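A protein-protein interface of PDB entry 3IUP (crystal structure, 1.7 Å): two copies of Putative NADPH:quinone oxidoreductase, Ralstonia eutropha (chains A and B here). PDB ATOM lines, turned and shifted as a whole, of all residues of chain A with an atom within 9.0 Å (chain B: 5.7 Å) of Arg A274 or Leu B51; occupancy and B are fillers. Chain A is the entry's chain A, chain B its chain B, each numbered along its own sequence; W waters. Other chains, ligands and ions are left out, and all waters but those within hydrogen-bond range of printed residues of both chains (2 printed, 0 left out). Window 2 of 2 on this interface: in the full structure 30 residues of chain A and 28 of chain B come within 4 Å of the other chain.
Arg A274 touches just these residues of chain B: Ser B47, Gly B50 and Leu B51. Printed residues of chain A within 4 Å of Leu B51: Arg A274. Of chain A, only Arg A274 comes within 4 Å of Gly B50. Of the printed residues of chain A, Arg B87 touches Tyr A272. Printed residues of chain B within 4 Å of Tyr A275: Ser B47. Of the printed residues of chain A, Ser B47 touches Arg A274 (3.0 Å) and Tyr A275 (3.2 Å). The nearest printed residue of chain A that does not touch Ser B47 is Tyr A272 (8.9 Å).
Hydrophobic or aromatic side chains of chain A that line the printed part of chain B: Tyr A272 and Tyr A275. Among the printed residues, 5 pairs touch across the chains.
The backbone carbonyl oxygen (O) of Leu B51 is in hydrogen-bond range of the side-chain hydroxyl (OG) of Ser B10 (3.3 Å). The guanidinium group of Arg B87 lies within hydrogen-bond range of the side-chain hydroxyl of Ser B10, at 2.8 Å. O of Leu B51 is in hydrogen-bond range of NH1 of Arg B87, 2.8 Å away. The backbone NH (N) of Met A302 sits at hydrogen-bond distance from the backbone carbonyl oxygen (O) of Tyr A275 (3.2 Å).
NH1 of Arg A274 is in hydrogen-bond range of O of Ser B47, at 3.0 Å.
Water W1 lies within hydrogen-bond range of the guanidinium group of Arg B87 (2.8 Å), the side-chain hydroxyl of Tyr A272 (3.3 Å) and the backbone carbonyl oxygen of Gly B50 (3.5 Å). Water W2 lies within hydrogen-bond range of the backbone carbonyl oxygen of Ser B47 (3.1 Å) and the guanidinium group of Arg A274 (3.1 Å).
Tyr A272 touches Arg B87 (CD1 to N, 3.7 Å). Arg A274 touches Gly B50. Leu B51 touches Arg A274. Tyr A275 touches Ser B47.
No position is printed for both chains.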
ATOM      1  N   GLU A 262     -20.033  15.188   6.428  1.00  0.00           N
ATOM      2  CA  GLU A 262     -18.834  14.973   5.620  1.00  0.00           C
ATOM      3  C   GLU A 262     -17.606  15.025   6.564  1.00  0.00           C
ATOM      4  O   GLU A 262     -16.680  14.237   6.392  1.00  0.00           O
ATOM      5  CB  GLU A 262     -18.741  16.000   4.514  1.00  0.00           C
ATOM      6  CG  GLU A 262     -17.554  15.856   3.605  1.00  0.00           C
ATOM      7  CD  GLU A 262     -17.555  14.620   2.709  1.00  0.00           C
ATOM      8  OE1 GLU A 262     -18.420  13.708   2.808  1.00  0.00           O
ATOM      9  OE2 GLU A 262     -16.606  14.553   1.886  1.00  0.00           O
ATOM     10  N   GLU A 271      -7.850   7.669   1.735  1.00  0.00           N
ATOM     11  CA  GLU A 271      -7.081   8.391   0.711  1.00  0.00           C
ATOM     12  C   GLU A 271      -7.535   9.844   0.652  1.00  0.00           C
ATOM     13  O   GLU A 271      -8.333  10.266   1.476  1.00  0.00           O
ATOM     14  CB  GLU A 271      -7.252   7.735  -0.665  1.00  0.00           C
ATOM     15  N   TYR A 272      -6.976  10.604  -0.282  1.00  0.00           N
ATOM     16  CA  TYR A 272      -7.471  11.954  -0.598  1.00  0.00           C
ATOM     17  C   TYR A 272      -8.424  11.849  -1.765  1.00  0.00           C
ATOM     18  O   TYR A 272      -8.032  11.422  -2.870  1.00  0.00           O
ATOM     19  CB  TYR A 272      -6.360  12.935  -1.000  1.00  0.00           C
ATOM     20  CG  TYR A 272      -6.880  14.336  -1.407  1.00  0.00           C
ATOM     21  CD1 TYR A 272      -7.544  15.152  -0.489  1.00  0.00           C
ATOM     22  CD2 TYR A 272      -6.710  14.836  -2.697  1.00  0.00           C
ATOM     23  CE1 TYR A 272      -8.015  16.427  -0.840  1.00  0.00           C
ATOM     24  CE2 TYR A 272      -7.188  16.114  -3.063  1.00  0.00           C
ATOM     25  CZ  TYR A 272      -7.841  16.906  -2.127  1.00  0.00           C
ATOM     26  OH  TYR A 272      -8.322  18.175  -2.456  1.00  0.00           O
ATOM     27  N   SER A 273      -9.672  12.242  -1.541  1.00  0.00           N
ATOM     28  CA  SER A 273     -10.629  12.288  -2.625  1.00  0.00           C
ATOM     29  C   SER A 273     -10.735  13.752  -3.040  1.00  0.00           C
ATOM     30  O   SER A 273     -11.090  14.644  -2.261  1.00  0.00           O
ATOM     31  CB  SER A 273     -11.983  11.692  -2.229  1.00  0.00           C
ATOM     32  N   ARG A 274     -10.378  13.993  -4.288  1.00  0.00           N
ATOM     33  CA  ARG A 274     -10.647  15.260  -4.951  1.00  0.00           C
ATOM     34  C   ARG A 274     -12.077  15.803  -4.632  1.00  0.00           C
ATOM     35  O   ARG A 274     -12.271  17.008  -4.411  1.00  0.00           O
ATOM     36  CB  ARG A 274     -10.414  14.989  -6.466  1.00  0.00           C
ATOM     37  CG  ARG A 274     -10.722  16.121  -7.433  1.00  0.00           C
ATOM     38  CD  ARG A 274      -9.671  17.220  -7.395  1.00  0.00           C
ATOM     39  NE  ARG A 274     -10.076  18.321  -8.280  1.00  0.00           N
ATOM     40  CZ  ARG A 274     -11.052  19.176  -7.997  1.00  0.00           C
ATOM     41  NH1 ARG A 274     -11.373  20.110  -8.846  1.00  0.00           N
ATOM     42  NH2 ARG A 274     -11.722  19.091  -6.846  1.00  0.00           N
ATOM     43  N   TYR A 275     -13.065  14.907  -4.572  1.00  0.00           N
ATOM     44  CA  TYR A 275     -14.486  15.277  -4.402  1.00  0.00           C
ATOM     45  C   TYR A 275     -15.113  14.841  -3.063  1.00  0.00           C
ATOM     46  O   TYR A 275     -16.368  14.689  -2.940  1.00  0.00           O
ATOM     47  CB  TYR A 275     -15.282  14.689  -5.564  1.00  0.00           C
ATOM     48  CG  TYR A 275     -14.772  15.239  -6.880  1.00  0.00           C
ATOM     49  CD1 TYR A 275     -14.989  16.585  -7.207  1.00  0.00           C
ATOM     50  CD2 TYR A 275     -14.077  14.437  -7.785  1.00  0.00           C
ATOM     51  CE1 TYR A 275     -14.520  17.121  -8.395  1.00  0.00           C
ATOM     52  CE2 TYR A 275     -13.613  14.965  -9.016  1.00  0.00           C
ATOM     53  CZ  TYR A 275     -13.836  16.315  -9.300  1.00  0.00           C
ATOM     54  OH  TYR A 275     -13.387  16.905 -10.475  1.00  0.00           O
ATOM     55  N   GLY A 276     -14.250  14.614  -2.073  1.00  0.00           N
ATOM     56  CA  GLY A 276     -14.699  14.191  -0.758  1.00  0.00           C
ATOM     57  C   GLY A 276     -15.129  12.721  -0.698  1.00  0.00           C
ATOM     58  O   GLY A 276     -14.789  11.905  -1.554  1.00  0.00           O
ATOM     59  N   SER A 277     -15.858  12.395   0.368  1.00  0.00           N
ATOM     60  CA  SER A 277     -16.247  11.013   0.659  1.00  0.00           C
ATOM     61  C   SER A 277     -17.147  10.579  -0.453  1.00  0.00           C
ATOM     62  O   SER A 277     -17.928  11.400  -0.979  1.00  0.00           O
ATOM     63  CB  SER A 277     -17.037  10.923   1.975  1.00  0.00           C
ATOM     64  OG  SER A 277     -17.541   9.613   2.176  1.00  0.00           O
ATOM     65  N   THR A 278     -17.122   9.290  -0.772  1.00  0.00           N
ATOM     66  CA  THR A 278     -18.090   8.764  -1.734  1.00  0.00           C
ATOM     67  C   THR A 278     -19.409   8.347  -1.112  1.00  0.00           C
ATOM     68  O   THR A 278     -20.337   8.000  -1.827  1.00  0.00           O
ATOM     69  CB  THR A 278     -17.529   7.540  -2.500  1.00  0.00           C
ATOM     70  OG1 THR A 278     -17.211   6.539  -1.548  1.00  0.00           O
ATOM     71  CG2 THR A 278     -16.276   7.941  -3.285  1.00  0.00           C
ATOM     72  N   PHE A 300     -18.938  19.905   1.377  1.00  0.00           N
ATOM     73  CA  PHE A 300     -19.197  18.551   1.758  1.00  0.00           C
ATOM     74  C   PHE A 300     -19.087  17.574   0.586  1.00  0.00           C
ATOM     75  O   PHE A 300     -19.593  16.473   0.623  1.00  0.00           O
ATOM     76  CB  PHE A 300     -20.553  18.481   2.485  1.00  0.00           C
ATOM     77  CG  PHE A 300     -21.666  19.293   1.840  1.00  0.00           C
ATOM     78  CD1 PHE A 300     -22.242  18.900   0.644  1.00  0.00           C
ATOM     79  CD2 PHE A 300     -22.151  20.455   2.439  1.00  0.00           C
ATOM     80  CE1 PHE A 300     -23.282  19.661   0.075  1.00  0.00           C
ATOM     81  CE2 PHE A 300     -23.162  21.187   1.874  1.00  0.00           C
ATOM     82  CZ  PHE A 300     -23.731  20.799   0.697  1.00  0.00           C
ATOM     83  N   GLY A 301     -18.342  17.956  -0.441  1.00  0.00           N
ATOM     84  CA  GLY A 301     -18.086  17.061  -1.553  1.00  0.00           C
ATOM     85  C   GLY A 301     -19.277  16.965  -2.485  1.00  0.00           C
ATOM     86  O   GLY A 301     -20.159  17.809  -2.456  1.00  0.00           O
ATOM     87  N   MET A 302     -19.281  15.919  -3.298  1.00  0.00           N
ATOM     88  CA  MET A 302     -20.234  15.763  -4.382  1.00  0.00           C
ATOM     89  C   MET A 302     -21.306  14.723  -4.099  1.00  0.00           C
ATOM     90  O   MET A 302     -22.297  14.650  -4.813  1.00  0.00           O
ATOM     91  CB  MET A 302     -19.461  15.418  -5.658  1.00  0.00           C
ATOM     92  CG  MET A 302     -18.382  16.445  -5.982  1.00  0.00           C
ATOM     93  SD  MET A 302     -19.253  18.099  -6.447  1.00  0.00           S
ATOM     94  CE  MET A 302     -20.035  17.438  -8.067  1.00  0.00           C
ATOM     95  N   SER B  10       1.853  19.786  -7.987  1.00  0.00           N
ATOM     96  CA  SER B  10       1.231  20.825  -7.185  1.00  0.00           C
ATOM     97  C   SER B  10       1.309  20.369  -5.735  1.00  0.00           C
ATOM     98  O   SER B  10       0.760  19.358  -5.398  1.00  0.00           O
ATOM     99  CB  SER B  10      -0.217  21.004  -7.600  1.00  0.00           C
ATOM    100  OG  SER B  10      -0.931  21.874  -6.732  1.00  0.00           O
ATOM    101  N   PRO B  46     -11.770  22.843 -15.690  1.00  0.00           N
ATOM    102  CA  PRO B  46     -11.993  23.313 -14.290  1.00  0.00           C
ATOM    103  C   PRO B  46     -11.632  22.330 -13.204  1.00  0.00           C
ATOM    104  O   PRO B  46     -11.083  22.765 -12.176  1.00  0.00           O
ATOM    105  CB  PRO B  46     -13.487  23.642 -14.272  1.00  0.00           C
ATOM    106  CG  PRO B  46     -13.783  23.989 -15.687  1.00  0.00           C
ATOM    107  CD  PRO B  46     -12.976  22.989 -16.513  1.00  0.00           C
ATOM    108  N   SER B  47     -11.861  21.023 -13.388  1.00  0.00           N
ATOM    109  CA  SER B  47     -11.491  20.055 -12.390  1.00  0.00           C
ATOM    110  C   SER B  47      -9.965  20.006 -12.214  1.00  0.00           C
ATOM    111  O   SER B  47      -9.454  19.851 -11.098  1.00  0.00           O
ATOM    112  CB  SER B  47     -12.046  18.657 -12.729  1.00  0.00           C
ATOM    113  OG  SER B  47     -11.744  18.349 -14.101  1.00  0.00           O
ATOM    114  N   ASP B  48      -9.228  20.172 -13.305  1.00  0.00           N
ATOM    115  CA  ASP B  48      -7.781  20.212 -13.235  1.00  0.00           C
ATOM    116  C   ASP B  48      -7.304  21.472 -12.522  1.00  0.00           C
ATOM    117  O   ASP B  48      -6.359  21.407 -11.761  1.00  0.00           O
ATOM    118  CB  ASP B  48      -7.186  20.186 -14.635  1.00  0.00           C
ATOM    119  CG  ASP B  48      -7.634  18.926 -15.432  1.00  0.00           C
ATOM    120  OD1 ASP B  48      -7.447  17.818 -14.888  1.00  0.00           O
ATOM    121  OD2 ASP B  48      -8.212  19.075 -16.535  1.00  0.00           O
ATOM    122  N   LEU B  49      -7.963  22.602 -12.781  1.00  0.00           N
ATOM    123  CA  LEU B  49      -7.576  23.890 -12.154  1.00  0.00           C
ATOM    124  C   LEU B  49      -7.777  23.783 -10.654  1.00  0.00           C
ATOM    125  O   LEU B  49      -6.993  24.346  -9.874  1.00  0.00           O
ATOM    126  CB  LEU B  49      -8.426  25.067 -12.718  1.00  0.00           C
ATOM    127  CG  LEU B  49      -8.267  25.254 -14.229  1.00  0.00           C
ATOM    128  CD1 LEU B  49      -9.175  26.339 -14.810  1.00  0.00           C
ATOM    129  CD2 LEU B  49      -6.827  25.561 -14.547  1.00  0.00           C
ATOM    130  N   GLY B  50      -8.832  23.097 -10.237  1.00  0.00           N
ATOM    131  CA  GLY B  50      -9.101  22.861  -8.858  1.00  0.00           C
ATOM    132  C   GLY B  50      -7.927  22.182  -8.184  1.00  0.00           C
ATOM    133  O   GLY B  50      -7.475  22.600  -7.123  1.00  0.00           O
ATOM    134  N   LEU B  51      -7.396  21.138  -8.814  1.00  0.00           N
ATOM    135  CA  LEU B  51      -6.255  20.441  -8.239  1.00  0.00           C
ATOM    136  C   LEU B  51      -4.958  21.221  -8.392  1.00  0.00           C
ATOM    137  O   LEU B  51      -4.106  21.203  -7.487  1.00  0.00           O
ATOM    138  CB  LEU B  51      -6.115  19.044  -8.896  1.00  0.00           C
ATOM    139  CG  LEU B  51      -5.060  18.111  -8.336  1.00  0.00           C
ATOM    140  CD1 LEU B  51      -5.347  17.862  -6.853  1.00  0.00           C
ATOM    141  CD2 LEU B  51      -5.054  16.787  -9.161  1.00  0.00           C
ATOM    142  N   LEU B  52      -4.777  21.873  -9.533  1.00  0.00           N
ATOM    143  CA  LEU B  52      -3.588  22.618  -9.779  1.00  0.00           C
ATOM    144  C   LEU B  52      -3.313  23.703  -8.727  1.00  0.00           C
ATOM    145  O   LEU B  52      -2.214  23.774  -8.160  1.00  0.00           O
ATOM    146  CB  LEU B  52      -3.692  23.250 -11.155  1.00  0.00           C
ATOM    147  CG  LEU B  52      -2.471  23.907 -11.720  1.00  0.00           C
ATOM    148  CD1 LEU B  52      -1.300  22.895 -11.817  1.00  0.00           C
ATOM    149  CD2 LEU B  52      -2.873  24.406 -13.124  1.00  0.00           C
ATOM    150  N   PHE B  53      -4.317  24.529  -8.456  1.00  0.00           N
ATOM    151  CA  PHE B  53      -4.120  25.671  -7.554  1.00  0.00           C
ATOM    152  C   PHE B  53      -4.686  25.416  -6.152  1.00  0.00           C
ATOM    153  O   PHE B  53      -4.392  26.180  -5.209  1.00  0.00           O
ATOM    154  CB  PHE B  53      -4.746  26.933  -8.150  1.00  0.00           C
ATOM    155  CG  PHE B  53      -4.270  27.239  -9.527  1.00  0.00           C
ATOM    156  CD1 PHE B  53      -2.936  27.362  -9.782  1.00  0.00           C
ATOM    157  CD2 PHE B  53      -5.156  27.366 -10.576  1.00  0.00           C
ATOM    158  CE1 PHE B  53      -2.455  27.665 -11.078  1.00  0.00           C
ATOM    159  CE2 PHE B  53      -4.696  27.640 -11.842  1.00  0.00           C
ATOM    160  CZ  PHE B  53      -3.342  27.789 -12.088  1.00  0.00           C
ATOM    161  N   GLY B  54      -5.467  24.341  -5.999  1.00  0.00           N
ATOM    162  CA  GLY B  54      -6.191  24.113  -4.755  1.00  0.00           C
ATOM    163  C   GLY B  54      -6.892  25.409  -4.340  1.00  0.00           C
ATOM    164  O   GLY B  54      -7.484  26.120  -5.170  1.00  0.00           O
ATOM    165  N   ARG B  87      -4.664  16.664   1.274  1.00  0.00           N
ATOM    166  CA  ARG B  87      -3.510  16.734   0.392  1.00  0.00           C
ATOM    167  C   ARG B  87      -2.329  17.495   0.977  1.00  0.00           C
ATOM    168  O   ARG B  87      -1.366  17.754   0.272  1.00  0.00           O
ATOM    169  CB  ARG B  87      -3.910  17.346  -0.966  1.00  0.00           C
ATOM    170  CG  ARG B  87      -4.415  18.745  -0.899  1.00  0.00           C
ATOM    171  CD  ARG B  87      -4.666  19.354  -2.265  1.00  0.00           C
ATOM    172  NE  ARG B  87      -3.412  19.487  -3.008  1.00  0.00           N
ATOM    173  CZ  ARG B  87      -3.291  20.139  -4.159  1.00  0.00           C
ATOM    174  NH1 ARG B  87      -4.352  20.676  -4.752  1.00  0.00           N
ATOM    175  NH2 ARG B  87      -2.114  20.242  -4.750  1.00  0.00           N
ATOM    176  N   MET B  92       1.272  16.463  -5.689  1.00  0.00           N
ATOM    177  CA  MET B  92       0.176  15.933  -6.511  1.00  0.00           C
ATOM    178  C   MET B  92       0.489  16.111  -7.991  1.00  0.00           C
ATOM    179  O   MET B  92       0.728  17.223  -8.463  1.00  0.00           O
ATOM    180  CB  MET B  92      -1.119  16.638  -6.187  1.00  0.00           C
ATOM    181  CG  MET B  92      -1.532  16.672  -4.762  1.00  0.00           C
ATOM    182  SD  MET B  92      -1.938  14.910  -4.122  1.00  0.00           S
ATOM    183  CE  MET B  92      -3.284  14.478  -5.487  1.00  0.00           C
ATOM    184  N   PRO B  93       0.498  15.020  -8.756  1.00  0.00           N
ATOM    185  CA  PRO B  93       0.437  15.166 -10.216  1.00  0.00           C
ATOM    186  C   PRO B  93      -0.918  15.710 -10.648  1.00  0.00           C
ATOM    187  O   PRO B  93      -1.880  15.632  -9.888  1.00  0.00           O
ATOM    188  CB  PRO B  93       0.590  13.732 -10.727  1.00  0.00           C
ATOM    189  CG  PRO B  93       0.748  12.866  -9.564  1.00  0.00           C
ATOM    190  CD  PRO B  93       0.410  13.620  -8.324  1.00  0.00           C
ATOM    191  N   VAL B  94      -1.009  16.290 -11.842  1.00  0.00           N
ATOM    192  CA  VAL B  94      -2.220  16.981 -12.272  1.00  0.00           C
ATOM    193  C   VAL B  94      -2.527  16.606 -13.684  1.00  0.00           C
ATOM    194  O   VAL B  94      -1.618  16.285 -14.443  1.00  0.00           O
ATOM    195  CB  VAL B  94      -2.072  18.535 -12.130  1.00  0.00           C
ATOM    196  CG1 VAL B  94      -3.437  19.248 -12.423  1.00  0.00           C
ATOM    197  CG2 VAL B  94      -1.571  18.843 -10.686  1.00  0.00           C
ATOM    198  N   GLY B  95      -3.812  16.626 -14.019  1.00  0.00           N
ATOM    199  CA  GLY B  95      -4.287  16.457 -15.362  1.00  0.00           C
ATOM    200  C   GLY B  95      -5.050  15.146 -15.509  1.00  0.00           C
ATOM    201  O   GLY B  95      -4.435  14.066 -15.534  1.00  0.00           O
HETATM  202  O   HOH W   1      -7.156  20.641  -4.264  1.00  0.00           O
HETATM  203  O   HOH W   2      -8.550  16.941 -10.593  1.00  0.00           O
